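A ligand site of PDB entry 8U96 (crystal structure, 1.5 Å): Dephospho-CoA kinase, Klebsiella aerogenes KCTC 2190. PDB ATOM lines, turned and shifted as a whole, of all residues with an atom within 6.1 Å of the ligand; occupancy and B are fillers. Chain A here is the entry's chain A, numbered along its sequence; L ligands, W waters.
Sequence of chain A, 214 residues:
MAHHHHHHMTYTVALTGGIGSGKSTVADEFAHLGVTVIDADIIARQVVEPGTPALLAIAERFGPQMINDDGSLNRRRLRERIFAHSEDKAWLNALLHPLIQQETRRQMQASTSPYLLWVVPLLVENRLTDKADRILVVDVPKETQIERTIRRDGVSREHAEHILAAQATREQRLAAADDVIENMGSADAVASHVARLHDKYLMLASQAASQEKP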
ATOM      1  N   GLY A  17       9.415  -1.030   6.522  1.00  0.00           N
ATOM      2  CA  GLY A  17       9.385  -0.204   7.706  1.00  0.00           C
ATOM      3  C   GLY A  17       9.391  -1.096   8.922  1.00  0.00           C
ATOM      4  O   GLY A  17       9.032  -2.280   8.853  1.00  0.00           O
ATOM      5  N   GLY A  18       9.795  -0.524  10.056  1.00  0.00           N
ATOM      6  CA  GLY A  18       9.880  -1.252  11.305  1.00  0.00           C
ATOM      7  C   GLY A  18       8.505  -1.510  11.913  1.00  0.00           C
ATOM      8  O   GLY A  18       7.474  -1.023  11.444  1.00  0.00           O
ATOM      9  N   ILE A  19       8.502  -2.308  12.977  1.00  0.00           N
ATOM     10  CA  ILE A  19       7.244  -2.600  13.654  1.00  0.00           C
ATOM     11  C   ILE A  19       6.567  -1.298  14.091  1.00  0.00           C
ATOM     12  O   ILE A  19       7.199  -0.362  14.596  1.00  0.00           O
ATOM     13  CB  ILE A  19       7.493  -3.550  14.853  1.00  0.00           C
ATOM     14  CG1 ILE A  19       6.148  -4.058  15.377  1.00  0.00           C
ATOM     15  CG2 ILE A  19       8.281  -2.850  15.937  1.00  0.00           C
ATOM     16  CD1 ILE A  19       6.265  -5.233  16.308  1.00  0.00           C
ATOM     17  N   GLY A  20       5.251  -1.252  13.872  1.00  0.00           N
ATOM     18  CA  GLY A  20       4.463  -0.111  14.286  1.00  0.00           C
ATOM     19  C   GLY A  20       4.568   1.117  13.400  1.00  0.00           C
ATOM     20  O   GLY A  20       3.979   2.142  13.739  1.00  0.00           O
ATOM     21  N   SER A  21       5.330   1.076  12.302  1.00  0.00           N
ATOM     22  CA  SER A  21       5.561   2.266  11.496  1.00  0.00           C
ATOM     23  C   SER A  21       4.360   2.614  10.620  1.00  0.00           C
ATOM     24  O   SER A  21       4.163   3.794  10.283  1.00  0.00           O
ATOM     25  CB  SER A  21       6.811   2.083  10.635  1.00  0.00           C
ATOM     26  OG  SER A  21       6.713   0.931   9.803  1.00  0.00           O
ATOM     27  N   GLY A  22       3.558   1.619  10.234  1.00  0.00           N
ATOM     28  CA  GLY A  22       2.383   1.858   9.406  1.00  0.00           C
ATOM     29  C   GLY A  22       2.505   1.359   7.984  1.00  0.00           C
ATOM     30  O   GLY A  22       1.919   1.964   7.077  1.00  0.00           O
ATOM     31  N   LYS A  23       3.254   0.287   7.760  1.00  0.00           N
ATOM     32  CA  LYS A  23       3.335  -0.309   6.433  1.00  0.00           C
ATOM     33  C   LYS A  23       1.943  -0.569   5.865  1.00  0.00           C
ATOM     34  O   LYS A  23       1.614  -0.086   4.768  1.00  0.00           O
ATOM     35  CB  LYS A  23       4.136  -1.618   6.487  1.00  0.00           C
ATOM     36  CG  LYS A  23       5.632  -1.450   6.813  1.00  0.00           C
ATOM     37  CD  LYS A  23       6.342  -2.804   6.941  1.00  0.00           C
ATOM     38  CE  LYS A  23       5.919  -3.551   8.172  1.00  0.00           C
ATOM     39  NZ  LYS A  23       6.203  -2.777   9.419  1.00  0.00           N
ATOM     40  N   SER A  24       1.094  -1.292   6.596  1.00  0.00           N
ATOM     41  CA  SER A  24      -0.246  -1.594   6.083  1.00  0.00           C
ATOM     42  C   SER A  24      -1.084  -0.340   5.935  1.00  0.00           C
ATOM     43  O   SER A  24      -1.876  -0.219   4.984  1.00  0.00           O
ATOM     44  CB  SER A  24      -0.950  -2.590   7.010  1.00  0.00           C
ATOM     45  OG  SER A  24      -0.271  -3.835   7.024  1.00  0.00           O
ATOM     46  N   THR A  25      -0.934   0.612   6.851  1.00  0.00           N
ATOM     47  CA  THR A  25      -1.678   1.854   6.763  1.00  0.00           C
ATOM     48  C   THR A  25      -1.366   2.618   5.469  1.00  0.00           C
ATOM     49  O   THR A  25      -2.270   3.127   4.782  1.00  0.00           O
ATOM     50  CB  THR A  25      -1.357   2.713   7.985  1.00  0.00           C
ATOM     51  OG1 THR A  25      -1.673   1.986   9.187  1.00  0.00           O
ATOM     52  CG2 THR A  25      -2.145   3.987   7.942  1.00  0.00           C
ATOM     53  N   VAL A  26      -0.091   2.722   5.125  1.00  0.00           N
ATOM     54  CA  VAL A  26       0.309   3.392   3.891  1.00  0.00           C
ATOM     55  C   VAL A  26      -0.076   2.562   2.659  1.00  0.00           C
ATOM     56  O   VAL A  26      -0.556   3.096   1.653  1.00  0.00           O
ATOM     57  CB  VAL A  26       1.822   3.674   3.929  1.00  0.00           C
ATOM     58  CG1 VAL A  26       2.355   4.050   2.556  1.00  0.00           C
ATOM     59  CG2 VAL A  26       2.115   4.775   4.965  1.00  0.00           C
ATOM     60  N   ASP A  41       1.423 -11.387   4.864  1.00  0.00           N
ATOM     61  CA  ASP A  41       0.705 -11.532   6.129  1.00  0.00           C
ATOM     62  C   ASP A  41      -0.803 -11.539   5.898  1.00  0.00           C
ATOM     63  O   ASP A  41      -1.536 -12.301   6.544  1.00  0.00           O
ATOM     64  CB  ASP A  41       1.083 -10.410   7.095  1.00  0.00           C
ATOM     65  CG  ASP A  41       2.531 -10.480   7.538  1.00  0.00           C
ATOM     66  OD1 ASP A  41       3.130 -11.574   7.493  1.00  0.00           O
ATOM     67  OD2 ASP A  41       3.081  -9.426   7.948  1.00  0.00           O
ATOM     68  N   VAL A 119       4.477  -5.430   0.109  1.00  0.00           N
ATOM     69  CA  VAL A 119       4.814  -5.135   1.501  1.00  0.00           C
ATOM     70  C   VAL A 119       5.819  -6.179   1.969  1.00  0.00           C
ATOM     71  O   VAL A 119       5.515  -7.376   2.007  1.00  0.00           O
ATOM     72  CB  VAL A 119       3.564  -5.111   2.389  1.00  0.00           C
ATOM     73  CG1 VAL A 119       3.931  -4.718   3.810  1.00  0.00           C
ATOM     74  CG2 VAL A 119       2.555  -4.148   1.846  1.00  0.00           C
ATOM     75  N   PRO A 121       8.171  -6.717   5.111  1.00  0.00           N
ATOM     76  CA  PRO A 121       8.658  -6.277   6.432  1.00  0.00           C
ATOM     77  C   PRO A 121      10.146  -6.455   6.665  1.00  0.00           C
ATOM     78  O   PRO A 121      10.772  -5.612   7.305  1.00  0.00           O
ATOM     79  CB  PRO A 121       7.824  -7.116   7.410  1.00  0.00           C
ATOM     80  CG  PRO A 121       7.293  -8.268   6.600  1.00  0.00           C
ATOM     81  CD  PRO A 121       7.069  -7.701   5.221  1.00  0.00           C
ATOM     82  N   ARG A 148       2.970   2.801  19.355  1.00  0.00           N
ATOM     83  CA  ARG A 148       1.941   2.173  18.537  1.00  0.00           C
ATOM     84  C   ARG A 148       1.931   0.657  18.693  1.00  0.00           C
ATOM     85  O   ARG A 148       0.864   0.032  18.593  1.00  0.00           O
ATOM     86  CB  ARG A 148       2.111   2.571  17.072  1.00  0.00           C
ATOM     87  CG  ARG A 148       1.881   4.067  16.822  1.00  0.00           C
ATOM     88  CD  ARG A 148       2.055   4.475  15.347  1.00  0.00           C
ATOM     89  NE  ARG A 148       2.008   5.920  15.210  1.00  0.00           N
ATOM     90  CZ  ARG A 148       2.221   6.575  14.079  1.00  0.00           C
ATOM     91  NH1 ARG A 148       2.442   5.936  12.937  1.00  0.00           N
ATOM     92  NH2 ARG A 148       2.220   7.906  14.090  1.00  0.00           N
ATOM     93  N   THR A 149       3.096   0.059  18.937  1.00  0.00           N
ATOM     94  CA  THR A 149       3.171  -1.384  19.152  1.00  0.00           C
ATOM     95  C   THR A 149       2.591  -1.773  20.501  1.00  0.00           C
ATOM     96  O   THR A 149       1.851  -2.770  20.596  1.00  0.00           O
ATOM     97  CB  THR A 149       4.633  -1.823  19.053  1.00  0.00           C
ATOM     98  OG1 THR A 149       5.149  -1.506  17.760  1.00  0.00           O
ATOM     99  CG2 THR A 149       4.745  -3.323  19.288  1.00  0.00           C
ATOM    100  N   ARG A 151       0.226  -0.216  22.052  1.00  0.00           N
ATOM    101  CA  ARG A 151      -1.227  -0.080  21.960  1.00  0.00           C
ATOM    102  C   ARG A 151      -1.852  -1.225  21.180  1.00  0.00           C
ATOM    103  O   ARG A 151      -2.905  -1.751  21.579  1.00  0.00           O
ATOM    104  CB  ARG A 151      -1.573   1.258  21.287  1.00  0.00           C
ATOM    105  CG  ARG A 151      -1.751   2.427  22.218  1.00  0.00           C
ATOM    106  CD  ARG A 151      -2.624   3.519  21.570  1.00  0.00           C
ATOM    107  NE  ARG A 151      -3.956   3.030  21.198  1.00  0.00           N
ATOM    108  CZ  ARG A 151      -4.346   2.702  19.971  1.00  0.00           C
ATOM    109  NH1 ARG A 151      -3.527   2.822  18.926  1.00  0.00           N
ATOM    110  NH2 ARG A 151      -5.571   2.235  19.784  1.00  0.00           N
ATOM    111  N   ARG A 152      -1.264  -1.578  20.047  1.00  0.00           N
ATOM    112  CA  ARG A 152      -1.891  -2.555  19.163  1.00  0.00           C
ATOM    113  C   ARG A 152      -1.758  -3.960  19.708  1.00  0.00           C
ATOM    114  O   ARG A 152      -2.707  -4.757  19.662  1.00  0.00           O
ATOM    115  CB  ARG A 152      -1.279  -2.480  17.770  1.00  0.00           C
ATOM    116  CG  ARG A 152      -2.003  -3.351  16.741  1.00  0.00           C
ATOM    117  CD  ARG A 152      -1.195  -3.457  15.460  1.00  0.00           C
ATOM    118  NE  ARG A 152       0.077  -4.133  15.681  1.00  0.00           N
ATOM    119  CZ  ARG A 152       1.102  -4.091  14.847  1.00  0.00           C
ATOM    120  NH1 ARG A 152       1.053  -3.386  13.728  1.00  0.00           N
ATOM    121  NH2 ARG A 152       2.210  -4.761  15.140  1.00  0.00           N
ATOM    122  N   ASP A 153      -0.582  -4.295  20.237  1.00  0.00           N
ATOM    123  CA  ASP A 153      -0.242  -5.668  20.564  1.00  0.00           C
ATOM    124  C   ASP A 153      -0.270  -5.985  22.049  1.00  0.00           C
ATOM    125  O   ASP A 153      -0.144  -7.160  22.412  1.00  0.00           O
ATOM    126  CB  ASP A 153       1.142  -6.005  20.007  1.00  0.00           C
ATOM    127  CG  ASP A 153       1.188  -5.988  18.509  1.00  0.00           C
ATOM    128  OD1 ASP A 153       0.106  -6.064  17.874  1.00  0.00           O
ATOM    129  OD2 ASP A 153       2.303  -5.925  17.948  1.00  0.00           O
ATOM    130  N   GLN A 167      15.315  -5.959  14.797  1.00  0.00           N
ATOM    131  CA  GLN A 167      15.038  -5.491  13.452  1.00  0.00           C
ATOM    132  C   GLN A 167      16.153  -4.555  13.002  1.00  0.00           C
ATOM    133  O   GLN A 167      16.977  -4.101  13.796  1.00  0.00           O
ATOM    134  CB  GLN A 167      13.690  -4.785  13.376  1.00  0.00           C
ATOM    135  CG  GLN A 167      12.530  -5.693  13.686  1.00  0.00           C
ATOM    136  CD  GLN A 167      11.186  -5.065  13.469  1.00  0.00           C
ATOM    137  OE1 GLN A 167      11.043  -3.835  13.472  1.00  0.00           O
ATOM    138  NE2 GLN A 167      10.168  -5.891  13.310  1.00  0.00           N
ATOM    139  N   ASN A 183       5.016   8.578   8.362  1.00  0.00           N
ATOM    140  CA  ASN A 183       3.622   8.328   8.737  1.00  0.00           C
ATOM    141  C   ASN A 183       3.343   9.044  10.049  1.00  0.00           C
ATOM    142  O   ASN A 183       3.095   8.445  11.116  1.00  0.00           O
ATOM    143  CB  ASN A 183       3.352   6.844   8.812  1.00  0.00           C
ATOM    144  CG  ASN A 183       1.912   6.520   9.186  1.00  0.00           C
ATOM    145  OD1 ASN A 183       0.984   7.293   8.897  1.00  0.00           O
ATOM    146  ND2 ASN A 183       1.711   5.363   9.818  1.00  0.00           N
ATOM    147  N   MET A 184       3.377  10.375   9.946  1.00  0.00           N
ATOM    148  CA  MET A 184       3.234  11.302  11.058  1.00  0.00           C
ATOM    149  C   MET A 184       2.421  12.498  10.597  1.00  0.00           C
ATOM    150  O   MET A 184       2.295  12.760   9.401  1.00  0.00           O
ATOM    151  CB  MET A 184       4.599  11.793  11.575  1.00  0.00           C
ATOM    152  CG  MET A 184       5.511  10.657  12.004  1.00  0.00           C
ATOM    153  SD  MET A 184       4.923   9.790  13.473  1.00  0.00           S
ATOM    154  CE  MET A 184       5.308  11.008  14.732  1.00  0.00           C
ATOM    155  N   GLY A 185       1.885  13.240  11.558  1.00  0.00           N
ATOM    156  CA  GLY A 185       1.076  14.410  11.252  1.00  0.00           C
ATOM    157  C   GLY A 185      -0.311  14.014  10.781  1.00  0.00           C
ATOM    158  O   GLY A 185      -0.799  12.922  11.046  1.00  0.00           O
ATOM    159  N   ALA A 187      -3.471  12.792   8.742  1.00  0.00           N
ATOM    160  CA  ALA A 187      -3.663  11.677   7.821  1.00  0.00           C
ATOM    161  C   ALA A 187      -3.877  12.162   6.384  1.00  0.00           C
ATOM    162  O   ALA A 187      -3.472  11.486   5.432  1.00  0.00           O
ATOM    163  CB  ALA A 187      -4.836  10.810   8.273  1.00  0.00           C
ATOM    164  N   VAL A 190      -0.467  12.708   4.797  1.00  0.00           N
ATOM    165  CA  VAL A 190       0.138  11.429   4.448  1.00  0.00           C
ATOM    166  C   VAL A 190      -0.471  10.887   3.161  1.00  0.00           C
ATOM    167  O   VAL A 190       0.244  10.443   2.254  1.00  0.00           O
ATOM    168  CB  VAL A 190       0.008  10.439   5.621  1.00  0.00           C
ATOM    169  CG1 VAL A 190       0.510   9.037   5.217  1.00  0.00           C
ATOM    170  CG2 VAL A 190       0.776  10.967   6.815  1.00  0.00           C
HETATM  171  P1  LIG L   1       3.830  -4.173  12.002  1.00  0.00           P
HETATM  172  O1  LIG L   1       4.007  -3.317  13.213  1.00  0.00           O
HETATM  173  O2  LIG L   1       3.125  -5.497  12.360  1.00  0.00           O
HETATM  174  O3  LIG L   1       5.130  -4.361  11.275  1.00  0.00           O
HETATM  175  P2  LIG L   1       2.763  -2.081  10.179  1.00  0.00           P
HETATM  176  O4  LIG L   1       4.052  -1.382  10.039  1.00  0.00           O
HETATM  177  O5  LIG L   1       1.994  -2.525   8.932  1.00  0.00           O
HETATM  178  O6  LIG L   1       2.870  -3.439  11.003  1.00  0.00           O
HETATM  179  P3  LIG L   1       0.242  -0.829  11.031  1.00  0.00           P
HETATM  180  O7  LIG L   1      -0.546  -2.036  11.398  1.00  0.00           O
HETATM  181  O8  LIG L   1      -0.065  -0.186   9.672  1.00  0.00           O
HETATM  182  O9  LIG L   1       1.776  -1.209  11.067  1.00  0.00           O
HETATM  183  O10 LIG L   1       0.133   0.307  12.128  1.00  0.00           O
HETATM  184  C1  LIG L   1       0.646   0.093  13.466  1.00  0.00           C
HETATM  185  C2  LIG L   1      -0.351   0.630  14.472  1.00  0.00           C
HETATM  186  O11 LIG L   1      -0.343   2.067  14.351  1.00  0.00           O
HETATM  187  C3  LIG L   1      -1.779   0.212  14.119  1.00  0.00           C
HETATM  188  O12 LIG L   1      -2.452   0.128  15.381  1.00  0.00           O
HETATM  189  C4  LIG L   1      -2.299   1.401  13.323  1.00  0.00           C
HETATM  190  O13 LIG L   1      -3.675   1.598  13.646  1.00  0.00           O
HETATM  191  C5  LIG L   1      -1.630   2.555  14.047  1.00  0.00           C
HETATM  192  N1  LIG L   1      -1.403   3.720  13.202  1.00  0.00           N
HETATM  193  C6  LIG L   1      -1.142   3.757  11.861  1.00  0.00           C
HETATM  194  N2  LIG L   1      -0.946   4.972  11.382  1.00  0.00           N
HETATM  195  C7  LIG L   1      -1.058   5.780  12.501  1.00  0.00           C
HETATM  196  C8  LIG L   1      -0.955   7.164  12.696  1.00  0.00           C
HETATM  197  N3  LIG L   1      -0.691   8.030  11.708  1.00  0.00           N
HETATM  198  N4  LIG L   1      -1.136   7.652  13.943  1.00  0.00           N
HETATM  199  C9  LIG L   1      -1.386   6.792  14.931  1.00  0.00           C
HETATM  200  N5  LIG L   1      -1.516   5.465  14.880  1.00  0.00           N
HETATM  201  C10 LIG L   1      -1.337   5.022  13.635  1.00  0.00           C
HETATM  202  O   HOH W   1       1.955   3.316  12.441  1.00  0.00           O
HETATM  203  O   HOH W   2      -1.638   8.223   8.412  1.00  0.00           O
HETATM  204  O   HOH W   3       7.517  -5.615  12.141  1.00  0.00           O
HETATM  205  O   HOH W   4      -4.805  -1.048  15.182  1.00  0.00           O
HETATM  206  O   HOH W   5      -1.861   4.231  17.530  1.00  0.00           O
HETATM  207  O   HOH W   6      -2.824  -2.723  11.764  1.00  0.00           O
HETATM  208  O   HOH W   7       1.017  -6.762  11.974  1.00  0.00           O
HETATM  209  O   HOH W   8      -0.368  -4.616  10.205  1.00  0.00           O
HETATM  210  O   HOH W   9      -1.478   1.434  17.612  1.00  0.00           O
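The backbone NH (N) of Gly 20 is in hydrogen-bond range of an oxygen (O1) of the ligand.
N of Lys 23 is in hydrogen-bond range of O4 of the ligand (2.9 Å).
An oxygen (O4) of the ligand is in salt-bridge range of the side-chain amino group (NZ) of Lys 23 (2.6 Å).
The backbone NH (N) of Thr 25 is in hydrogen-bond range of an oxygen (O8) of the ligand.
O8 of the ligand lies within hydrogen-bond range of OG1 of Thr 25, at 2.7 Å.
O5 of the ligand is in hydrogen-bond range of N of Ser 24, at 2.8 Å.
An oxygen (O5) of the ligand lies within hydrogen-bond range of the side-chain hydroxyl (OG) of Ser 24, 3.2 Å away.
The guanidinium group (NH1) of Arg 152 lies within salt-bridge range of an oxygen (O1) of the ligand (3.0 Å).
An oxygen (O4) of the ligand sits at hydrogen-bond distance from the backbone NH of Gly 22 (3.0 Å).
A nitrogen (N2) of the ligand is in hydrogen-bond range of the side-chain amide nitrogen (ND2) of Asn 183 (3.1 Å).
The guanidinium group of Arg 148 sits at hydrogen-bond distance from a nitrogen (N4) of the ligand (3.4 Å).
Water W9 lies within hydrogen-bond range of an oxygen (O12) of the ligand (2.8 Å), the guanidinium group of Arg 151 (2.8 Å) and the backbone carbonyl oxygen of Arg 148 (2.9 Å).
Water W3 bridges an oxygen (O3) of the ligand (2.8 Å) and the side-chain amide nitrogen of Gln 167 (2.9 Å).
Water W8 lies within hydrogen-bond range of O7 of the ligand (2.8 Å) and OG of Ser 24 (3.3 Å).
Water W5 lies within hydrogen-bond range of NH1 of Arg 151 (2.6 Å) and N5 of the ligand (2.9 Å).
Water W2 lies within hydrogen-bond range of the side-chain amide oxygen (OD1) of Asn 183 and a nitrogen (N3) of the ligand.
O of Gly 18 sits at hydrogen-bond distance from NZ of Lys 23, 3.0 Å away.
O of Gly 17 sits at hydrogen-bond distance from NZ of Lys 23 (2.9 Å).
The guanidinium group (NE) of Arg 152 is in salt-bridge range of the side-chain carboxylate (OD1) of Asp 153 (2.9 Å).
NH2 of Arg 148 is in hydrogen-bond range of O of Asn 183, 3.1 Å away.
The side-chain amide nitrogen of Asn 183 is in hydrogen-bond range of the backbone carbonyl oxygen of Ser 21 (2.9 Å).
N of Ile 19 is in hydrogen-bond range of OE1 of Gln 167, 3.0 Å away.
The guanidinium group (NH2) of Arg 148 is in hydrogen-bond range of the side-chain sulfur (SD) of Met 184, at 3.4 Å.
OG of Ser 21 is in hydrogen-bond range of O of Gly 18 (2.7 Å).
Gly 18 touches the ligand (O to O4, 3.7 Å).
Ile 19 touches the ligand (CG1 to O1, 3.1 Å).
OG of Ser 21 touches O4 of the ligand (3.5 Å).
Along chain A the residues within 4 Å of the ligand span positions 18 to 183.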
